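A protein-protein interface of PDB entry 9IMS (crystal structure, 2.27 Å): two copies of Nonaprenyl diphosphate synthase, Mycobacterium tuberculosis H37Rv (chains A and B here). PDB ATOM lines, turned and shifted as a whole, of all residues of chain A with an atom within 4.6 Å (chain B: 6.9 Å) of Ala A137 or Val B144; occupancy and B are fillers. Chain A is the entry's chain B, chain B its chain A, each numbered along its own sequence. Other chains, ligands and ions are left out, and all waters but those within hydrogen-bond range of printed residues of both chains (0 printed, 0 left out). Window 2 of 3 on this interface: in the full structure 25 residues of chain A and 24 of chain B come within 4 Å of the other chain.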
ATOM      1  N   SER A 133       8.271  23.947  -1.348  1.00  0.00           N
ATOM      2  CA  SER A 133       8.868  23.325  -2.537  1.00  0.00           C
ATOM      3  C   SER A 133       8.253  21.962  -2.809  1.00  0.00           C
ATOM      4  O   SER A 133       7.847  21.656  -3.936  1.00  0.00           O
ATOM      5  CB  SER A 133      10.382  23.152  -2.363  1.00  0.00           C
ATOM      6  OG  SER A 133      11.063  24.368  -2.546  1.00  0.00           O
ATOM      7  N   ARG A 134       8.195  21.123  -1.782  1.00  0.00           N
ATOM      8  CA  ARG A 134       7.640  19.791  -1.962  1.00  0.00           C
ATOM      9  C   ARG A 134       6.192  19.850  -2.434  1.00  0.00           C
ATOM     10  O   ARG A 134       5.788  19.092  -3.323  1.00  0.00           O
ATOM     11  CB  ARG A 134       7.762  19.004  -0.657  1.00  0.00           C
ATOM     12  CG  ARG A 134       7.134  17.624  -0.733  1.00  0.00           C
ATOM     13  CD  ARG A 134       7.586  16.765   0.434  1.00  0.00           C
ATOM     14  NE  ARG A 134       7.366  17.423   1.716  1.00  0.00           N
ATOM     15  CZ  ARG A 134       6.190  17.516   2.316  1.00  0.00           C
ATOM     16  NH1 ARG A 134       5.088  17.044   1.748  1.00  0.00           N
ATOM     17  NH2 ARG A 134       6.118  18.090   3.520  1.00  0.00           N
ATOM     18  N   LEU A 135       5.401  20.762  -1.876  1.00  0.00           N
ATOM     19  CA  LEU A 135       3.990  20.821  -2.258  1.00  0.00           C
ATOM     20  C   LEU A 135       3.822  21.358  -3.672  1.00  0.00           C
ATOM     21  O   LEU A 135       3.050  20.802  -4.464  1.00  0.00           O
ATOM     22  CB  LEU A 135       3.207  21.674  -1.261  1.00  0.00           C
ATOM     23  CG  LEU A 135       2.421  20.926  -0.185  1.00  0.00           C
ATOM     24  CD1 LEU A 135       3.282  19.872   0.471  1.00  0.00           C
ATOM     25  CD2 LEU A 135       1.898  21.908   0.870  1.00  0.00           C
ATOM     26  N   VAL A 136       4.527  22.438  -4.014  1.00  0.00           N
ATOM     27  CA  VAL A 136       4.316  23.025  -5.332  1.00  0.00           C
ATOM     28  C   VAL A 136       4.897  22.117  -6.406  1.00  0.00           C
ATOM     29  O   VAL A 136       4.364  22.052  -7.521  1.00  0.00           O
ATOM     30  CB  VAL A 136       4.892  24.453  -5.410  1.00  0.00           C
ATOM     31  CG1 VAL A 136       6.404  24.421  -5.560  1.00  0.00           C
ATOM     32  CG2 VAL A 136       4.261  25.234  -6.586  1.00  0.00           C
ATOM     33  N   ALA A 137       5.970  21.381  -6.082  1.00  0.00           N
ATOM     34  CA  ALA A 137       6.565  20.452  -7.037  1.00  0.00           C
ATOM     35  C   ALA A 137       5.524  19.484  -7.575  1.00  0.00           C
ATOM     36  O   ALA A 137       5.523  19.162  -8.768  1.00  0.00           O
ATOM     37  CB  ALA A 137       7.713  19.679  -6.383  1.00  0.00           C
ATOM     38  N   ARG A 138       4.606  19.030  -6.720  1.00  0.00           N
ATOM     39  CA  ARG A 138       3.612  18.090  -7.209  1.00  0.00           C
ATOM     40  C   ARG A 138       2.454  18.774  -7.910  1.00  0.00           C
ATOM     41  O   ARG A 138       1.643  18.086  -8.538  1.00  0.00           O
ATOM     42  CB  ARG A 138       3.101  17.200  -6.072  1.00  0.00           C
ATOM     43  CG  ARG A 138       2.156  17.866  -5.119  1.00  0.00           C
ATOM     44  CD  ARG A 138       2.387  17.306  -3.713  1.00  0.00           C
ATOM     45  NE  ARG A 138       1.200  17.413  -2.873  1.00  0.00           N
ATOM     46  CZ  ARG A 138       1.178  17.144  -1.575  1.00  0.00           C
ATOM     47  NH1 ARG A 138       2.247  16.675  -0.948  1.00  0.00           N
ATOM     48  NH2 ARG A 138       0.055  17.355  -0.888  1.00  0.00           N
ATOM     49  N   LEU A 139       2.366  20.099  -7.835  1.00  0.00           N
ATOM     50  CA  LEU A 139       1.452  20.834  -8.694  1.00  0.00           C
ATOM     51  C   LEU A 139       1.958  20.936 -10.134  1.00  0.00           C
ATOM     52  O   LEU A 139       1.149  21.162 -11.044  1.00  0.00           O
ATOM     53  CB  LEU A 139       1.214  22.238  -8.131  1.00  0.00           C
ATOM     54  CG  LEU A 139       0.415  22.342  -6.824  1.00  0.00           C
ATOM     55  CD1 LEU A 139       0.252  23.800  -6.379  1.00  0.00           C
ATOM     56  CD2 LEU A 139      -0.953  21.652  -6.935  1.00  0.00           C
ATOM     57  N   GLY A 140       3.265  20.785 -10.362  1.00  0.00           N
ATOM     58  CA  GLY A 140       3.795  20.786 -11.706  1.00  0.00           C
ATOM     59  C   GLY A 140       4.785  21.898 -11.991  1.00  0.00           C
ATOM     60  O   GLY A 140       4.839  22.911 -11.287  1.00  0.00           O
ATOM     61  N   PRO A 141       5.589  21.724 -13.051  1.00  0.00           N
ATOM     62  CA  PRO A 141       6.608  22.741 -13.376  1.00  0.00           C
ATOM     63  C   PRO A 141       6.059  24.141 -13.606  1.00  0.00           C
ATOM     64  O   PRO A 141       6.729  25.111 -13.236  1.00  0.00           O
ATOM     65  CB  PRO A 141       7.259  22.171 -14.645  1.00  0.00           C
ATOM     66  CG  PRO A 141       7.159  20.671 -14.422  1.00  0.00           C
ATOM     67  CD  PRO A 141       5.769  20.504 -13.857  1.00  0.00           C
ATOM     68  N   VAL A 144       5.491  25.558 -10.304  1.00  0.00           N
ATOM     69  CA  VAL A 144       6.807  25.829  -9.721  1.00  0.00           C
ATOM     70  C   VAL A 144       7.338  27.165 -10.217  1.00  0.00           C
ATOM     71  O   VAL A 144       7.807  28.003  -9.430  1.00  0.00           O
ATOM     72  CB  VAL A 144       7.800  24.688 -10.039  1.00  0.00           C
ATOM     73  CG1 VAL A 144       9.207  25.078  -9.599  1.00  0.00           C
ATOM     74  CG2 VAL A 144       7.378  23.386  -9.365  1.00  0.00           C
ATOM     75  N   SER B 133      14.897  27.622  -8.347  1.00  0.00           N
ATOM     76  CA  SER B 133      13.638  26.901  -8.494  1.00  0.00           C
ATOM     77  C   SER B 133      12.967  27.248  -9.814  1.00  0.00           C
ATOM     78  O   SER B 133      12.437  26.360 -10.494  1.00  0.00           O
ATOM     79  CB  SER B 133      12.710  27.205  -7.319  1.00  0.00           C
ATOM     80  OG  SER B 133      13.416  27.126  -6.101  1.00  0.00           O
ATOM     81  N   VAL B 136      14.947  25.270 -12.667  1.00  0.00           N
ATOM     82  CA  VAL B 136      14.761  23.824 -12.761  1.00  0.00           C
ATOM     83  C   VAL B 136      13.379  23.456 -13.295  1.00  0.00           C
ATOM     84  O   VAL B 136      13.194  22.348 -13.804  1.00  0.00           O
ATOM     85  CB  VAL B 136      15.012  23.130 -11.404  1.00  0.00           C
ATOM     86  CG1 VAL B 136      13.776  23.197 -10.514  1.00  0.00           C
ATOM     87  CG2 VAL B 136      15.409  21.687 -11.629  1.00  0.00           C
ATOM     88  N   ALA B 137      12.396  24.351 -13.189  1.00  0.00           N
ATOM     89  CA  ALA B 137      11.092  24.061 -13.771  1.00  0.00           C
ATOM     90  C   ALA B 137      11.206  23.796 -15.261  1.00  0.00           C
ATOM     91  O   ALA B 137      10.442  22.990 -15.807  1.00  0.00           O
ATOM     92  CB  ALA B 137      10.133  25.220 -13.515  1.00  0.00           C
ATOM     93  N   ARG B 138      12.164  24.452 -15.926  1.00  0.00           N
ATOM     94  CA  ARG B 138      12.409  24.200 -17.340  1.00  0.00           C
ATOM     95  C   ARG B 138      12.791  22.751 -17.603  1.00  0.00           C
ATOM     96  O   ARG B 138      12.565  22.241 -18.708  1.00  0.00           O
ATOM     97  CB  ARG B 138      13.518  25.112 -17.854  1.00  0.00           C
ATOM     98  CG  ARG B 138      13.288  26.579 -17.611  1.00  0.00           C
ATOM     99  CD  ARG B 138      14.322  27.383 -18.378  1.00  0.00           C
ATOM    100  NE  ARG B 138      14.235  28.808 -18.080  1.00  0.00           N
ATOM    101  CZ  ARG B 138      15.168  29.688 -18.404  1.00  0.00           C
ATOM    102  NH1 ARG B 138      16.231  29.337 -19.116  1.00  0.00           N
ATOM    103  NH2 ARG B 138      15.048  30.941 -17.980  1.00  0.00           N
ATOM    104  N   LEU B 139      13.382  22.078 -16.616  1.00  0.00           N
ATOM    105  CA  LEU B 139      13.858  20.720 -16.832  1.00  0.00           C
ATOM    106  C   LEU B 139      12.779  19.671 -16.623  1.00  0.00           C
ATOM    107  O   LEU B 139      13.062  18.487 -16.809  1.00  0.00           O
ATOM    108  CB  LEU B 139      15.053  20.417 -15.918  1.00  0.00           C
ATOM    109  CG  LEU B 139      16.329  21.249 -16.093  1.00  0.00           C
ATOM    110  CD1 LEU B 139      17.464  20.667 -15.243  1.00  0.00           C
ATOM    111  CD2 LEU B 139      16.740  21.383 -17.580  1.00  0.00           C
ATOM    112  N   GLY B 140      11.565  20.061 -16.232  1.00  0.00           N
ATOM    113  CA  GLY B 140      10.459  19.138 -16.210  1.00  0.00           C
ATOM    114  C   GLY B 140      10.164  18.569 -14.839  1.00  0.00           C
ATOM    115  O   GLY B 140      10.829  18.896 -13.851  1.00  0.00           O
ATOM    116  N   PRO B 141       9.169  17.672 -14.761  1.00  0.00           N
ATOM    117  CA  PRO B 141       8.647  17.272 -13.438  1.00  0.00           C
ATOM    118  C   PRO B 141       9.622  16.450 -12.624  1.00  0.00           C
ATOM    119  O   PRO B 141       9.655  16.586 -11.395  1.00  0.00           O
ATOM    120  CB  PRO B 141       7.386  16.459 -13.782  1.00  0.00           C
ATOM    121  CG  PRO B 141       7.127  16.689 -15.243  1.00  0.00           C
ATOM    122  CD  PRO B 141       8.443  17.025 -15.866  1.00  0.00           C
ATOM    123  N   GLU B 142      10.411  15.582 -13.268  1.00  0.00           N
ATOM    124  CA  GLU B 142      11.360  14.761 -12.521  1.00  0.00           C
ATOM    125  C   GLU B 142      12.450  15.622 -11.886  1.00  0.00           C
ATOM    126  O   GLU B 142      12.751  15.482 -10.693  1.00  0.00           O
ATOM    127  CB  GLU B 142      11.957  13.688 -13.433  1.00  0.00           C
ATOM    128  CG  GLU B 142      10.953  13.054 -14.447  1.00  0.00           C
ATOM    129  CD  GLU B 142      10.596  13.933 -15.691  1.00  0.00           C
ATOM    130  OE1 GLU B 142      11.048  15.098 -15.805  1.00  0.00           O
ATOM    131  OE2 GLU B 142       9.847  13.434 -16.565  1.00  0.00           O
ATOM    132  N   ALA B 143      13.031  16.545 -12.661  1.00  0.00           N
ATOM    133  CA  ALA B 143      14.049  17.436 -12.114  1.00  0.00           C
ATOM    134  C   ALA B 143      13.497  18.241 -10.949  1.00  0.00           C
ATOM    135  O   ALA B 143      14.179  18.444  -9.936  1.00  0.00           O
ATOM    136  CB  ALA B 143      14.562  18.377 -13.202  1.00  0.00           C
ATOM    137  N   VAL B 144      12.263  18.721 -11.087  1.00  0.00           N
ATOM    138  CA  VAL B 144      11.659  19.532 -10.041  1.00  0.00           C
ATOM    139  C   VAL B 144      11.594  18.744  -8.733  1.00  0.00           C
ATOM    140  O   VAL B 144      11.965  19.248  -7.664  1.00  0.00           O
ATOM    141  CB  VAL B 144      10.273  20.031 -10.504  1.00  0.00           C
ATOM    142  CG1 VAL B 144       9.380  20.262  -9.350  1.00  0.00           C
ATOM    143  CG2 VAL B 144      10.402  21.305 -11.335  1.00  0.00           C
ATOM    144  N   ARG B 145      11.159  17.481  -8.795  1.00  0.00           N
ATOM    145  CA  ARG B 145      11.096  16.690  -7.563  1.00  0.00           C
ATOM    146  C   ARG B 145      12.486  16.440  -6.981  1.00  0.00           C
ATOM    147  O   ARG B 145      12.663  16.442  -5.752  1.00  0.00           O
ATOM    148  CB  ARG B 145      10.377  15.358  -7.811  1.00  0.00           C
ATOM    149  CG  ARG B 145       8.966  15.490  -8.405  1.00  0.00           C
ATOM    150  CD  ARG B 145       8.339  14.104  -8.678  1.00  0.00           C
ATOM    151  NE  ARG B 145       7.773  13.990 -10.021  1.00  0.00           N
ATOM    152  CZ  ARG B 145       8.319  13.277 -11.006  1.00  0.00           C
ATOM    153  NH1 ARG B 145       9.459  12.617 -10.837  1.00  0.00           N
ATOM    154  NH2 ARG B 145       7.716  13.239 -12.196  1.00  0.00           N
ATOM    155  N   ILE B 146      13.489  16.257  -7.844  1.00  0.00           N
ATOM    156  CA  ILE B 146      14.842  16.031  -7.352  1.00  0.00           C
ATOM    157  C   ILE B 146      15.339  17.243  -6.579  1.00  0.00           C
ATOM    158  O   ILE B 146      15.983  17.113  -5.532  1.00  0.00           O
ATOM    159  CB  ILE B 146      15.771  15.679  -8.521  1.00  0.00           C
ATOM    160  CG1 ILE B 146      15.535  14.229  -8.939  1.00  0.00           C
ATOM    161  CG2 ILE B 146      17.219  15.929  -8.150  1.00  0.00           C
ATOM    162  CD1 ILE B 146      15.669  14.014 -10.439  1.00  0.00           C
ATOM    163  N   ILE B 147      15.049  18.444  -7.073  1.00  0.00           N
ATOM    164  CA  ILE B 147      15.505  19.623  -6.351  1.00  0.00           C
ATOM    165  C   ILE B 147      14.738  19.787  -5.041  1.00  0.00           C
ATOM    166  O   ILE B 147      15.339  20.073  -3.995  1.00  0.00           O
ATOM    167  CB  ILE B 147      15.403  20.864  -7.254  1.00  0.00           C
ATOM    168  CG1 ILE B 147      16.358  20.682  -8.425  1.00  0.00           C
ATOM    169  CG2 ILE B 147      15.771  22.120  -6.481  1.00  0.00           C
ATOM    170  CD1 ILE B 147      17.799  20.610  -7.980  1.00  0.00           C
ATOM    171  N   ALA B 148      13.411  19.583  -5.069  1.00  0.00           N
ATOM    172  CA  ALA B 148      12.625  19.733  -3.844  1.00  0.00           C
ATOM    173  C   ALA B 148      13.109  18.767  -2.768  1.00  0.00           C
ATOM    174  O   ALA B 148      13.244  19.138  -1.594  1.00  0.00           O
ATOM    175  CB  ALA B 148      11.130  19.523  -4.126  1.00  0.00           C
ATOM    176  N   ASP B 149      13.410  17.527  -3.159  1.00  0.00           N
ATOM    177  CA  ASP B 149      13.963  16.567  -2.211  1.00  0.00           C
ATOM    178  C   ASP B 149      15.336  16.998  -1.723  1.00  0.00           C
ATOM    179  O   ASP B 149      15.666  16.801  -0.549  1.00  0.00           O
ATOM    180  CB  ASP B 149      14.007  15.201  -2.872  1.00  0.00           C
ATOM    181  CG  ASP B 149      12.628  14.736  -3.267  1.00  0.00           C
ATOM    182  OD1 ASP B 149      12.497  13.721  -3.988  1.00  0.00           O
ATOM    183  OD2 ASP B 149      11.655  15.384  -2.812  1.00  0.00           O
ATOM    184  N   THR B 150      16.136  17.621  -2.586  1.00  0.00           N
ATOM    185  CA  THR B 150      17.433  18.126  -2.137  1.00  0.00           C
ATOM    186  C   THR B 150      17.264  19.240  -1.109  1.00  0.00           C
ATOM    187  O   THR B 150      17.959  19.263  -0.086  1.00  0.00           O
ATOM    188  CB  THR B 150      18.248  18.611  -3.337  1.00  0.00           C
ATOM    189  OG1 THR B 150      18.373  17.542  -4.282  1.00  0.00           O
ATOM    190  CG2 THR B 150      19.644  19.069  -2.903  1.00  0.00           C
ATOM    191  N   PHE B 151      16.347  20.185  -1.366  1.00  0.00           N
ATOM    192  CA  PHE B 151      16.053  21.210  -0.377  1.00  0.00           C
ATOM    193  C   PHE B 151      15.709  20.579   0.970  1.00  0.00           C
ATOM    194  O   PHE B 151      16.169  21.039   2.018  1.00  0.00           O
ATOM    195  CB  PHE B 151      14.894  22.096  -0.845  1.00  0.00           C
ATOM    196  CG  PHE B 151      15.235  23.032  -1.983  1.00  0.00           C
ATOM    197  CD1 PHE B 151      16.509  23.559  -2.127  1.00  0.00           C
ATOM    198  CD2 PHE B 151      14.257  23.397  -2.904  1.00  0.00           C
ATOM    199  CE1 PHE B 151      16.802  24.443  -3.171  1.00  0.00           C
ATOM    200  CE2 PHE B 151      14.552  24.280  -3.974  1.00  0.00           C
ATOM    201  CZ  PHE B 151      15.826  24.799  -4.097  1.00  0.00           C
ATOM    202  N   LEU B 193      21.272  14.812 -12.208  1.00  0.00           N
ATOM    203  CA  LEU B 193      20.801  15.603 -13.336  1.00  0.00           C
ATOM    204  C   LEU B 193      21.742  15.471 -14.527  1.00  0.00           C
ATOM    205  O   LEU B 193      21.287  15.453 -15.675  1.00  0.00           O
ATOM    206  CB  LEU B 193      20.660  17.060 -12.926  1.00  0.00           C
ATOM    207  CG  LEU B 193      19.576  17.342 -11.887  1.00  0.00           C
ATOM    208  CD1 LEU B 193      19.725  18.762 -11.362  1.00  0.00           C
ATOM    209  CD2 LEU B 193      18.199  17.096 -12.476  1.00  0.00           C
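Of the 10 printed residues of chain A, 4 touch a printed residue of chain B.
Hydrophobic or aromatic side chains of chain A within 4 Å of the printed part of chain B: Ala A137, Pro A141 and Val A144.
Hydrophobic or aromatic side chains of chain B that line the printed part of chain A: Ala B137, Val B144, Ala B148 and Phe B151.
Along chain B the printed residues that touch a printed residue of chain A span positions 133 to 151.
Among the printed residues, merely in contact across the chains: Ser A133 with Ala B148 (3.9 Å), Ser A133 with Phe B151 (3.4 Å), Ala A137 with Val B144 (3.5 Å), Pro A141 with Ala B137 (3.4 Å), Pro A141 with Gly B140 (3.7 Å), Pro A141 with Pro B141 (3.6 Å), Val A144 with Ser B133 (3.6 Å) and Val A144 with Val B144 (3.7 Å).
Ala A137 touches just one residue of chain B: Val B144 (3.5 Å).
Of the printed residues of chain A, Phe B151 touches Ser A133.
Of the printed residues of chain A, Pro B141 touches Pro A141 (3.6 Å).
Of the printed residues of chain A, Ala B148 touches Ser A133.
Printed residues of chain B within 4 Å of Val A144: Ser B133 (3.6 Å) and Val B144 (3.7 Å).
Printed residues of chain A within 4 Å of Gly B140: Pro A141.
The nearest residue of chain A that does not touch Val B144 is Pro A141 (4.5 Å).
The nearest printed residue of chain A that does not touch Ala B137 is Val A144 (4.03 Å).
Pro A141 touches Gly B140, but with the chains exchanged Gly A140 does not touch Pro B141 (6.0 Å).
Pro A141 touches its own counterpart, Pro B141.
Val A144 touches Ser B133, but with the chains exchanged Ser A133 does not touch Val B144 (5.8 Å).
Val B144 touches its own counterpart, Val A144.
8 positions are printed for both chains.
The guanidinium group of Arg B145 sits close to the backbone carbonyl oxygen of Pro B141 (3.5 Å).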
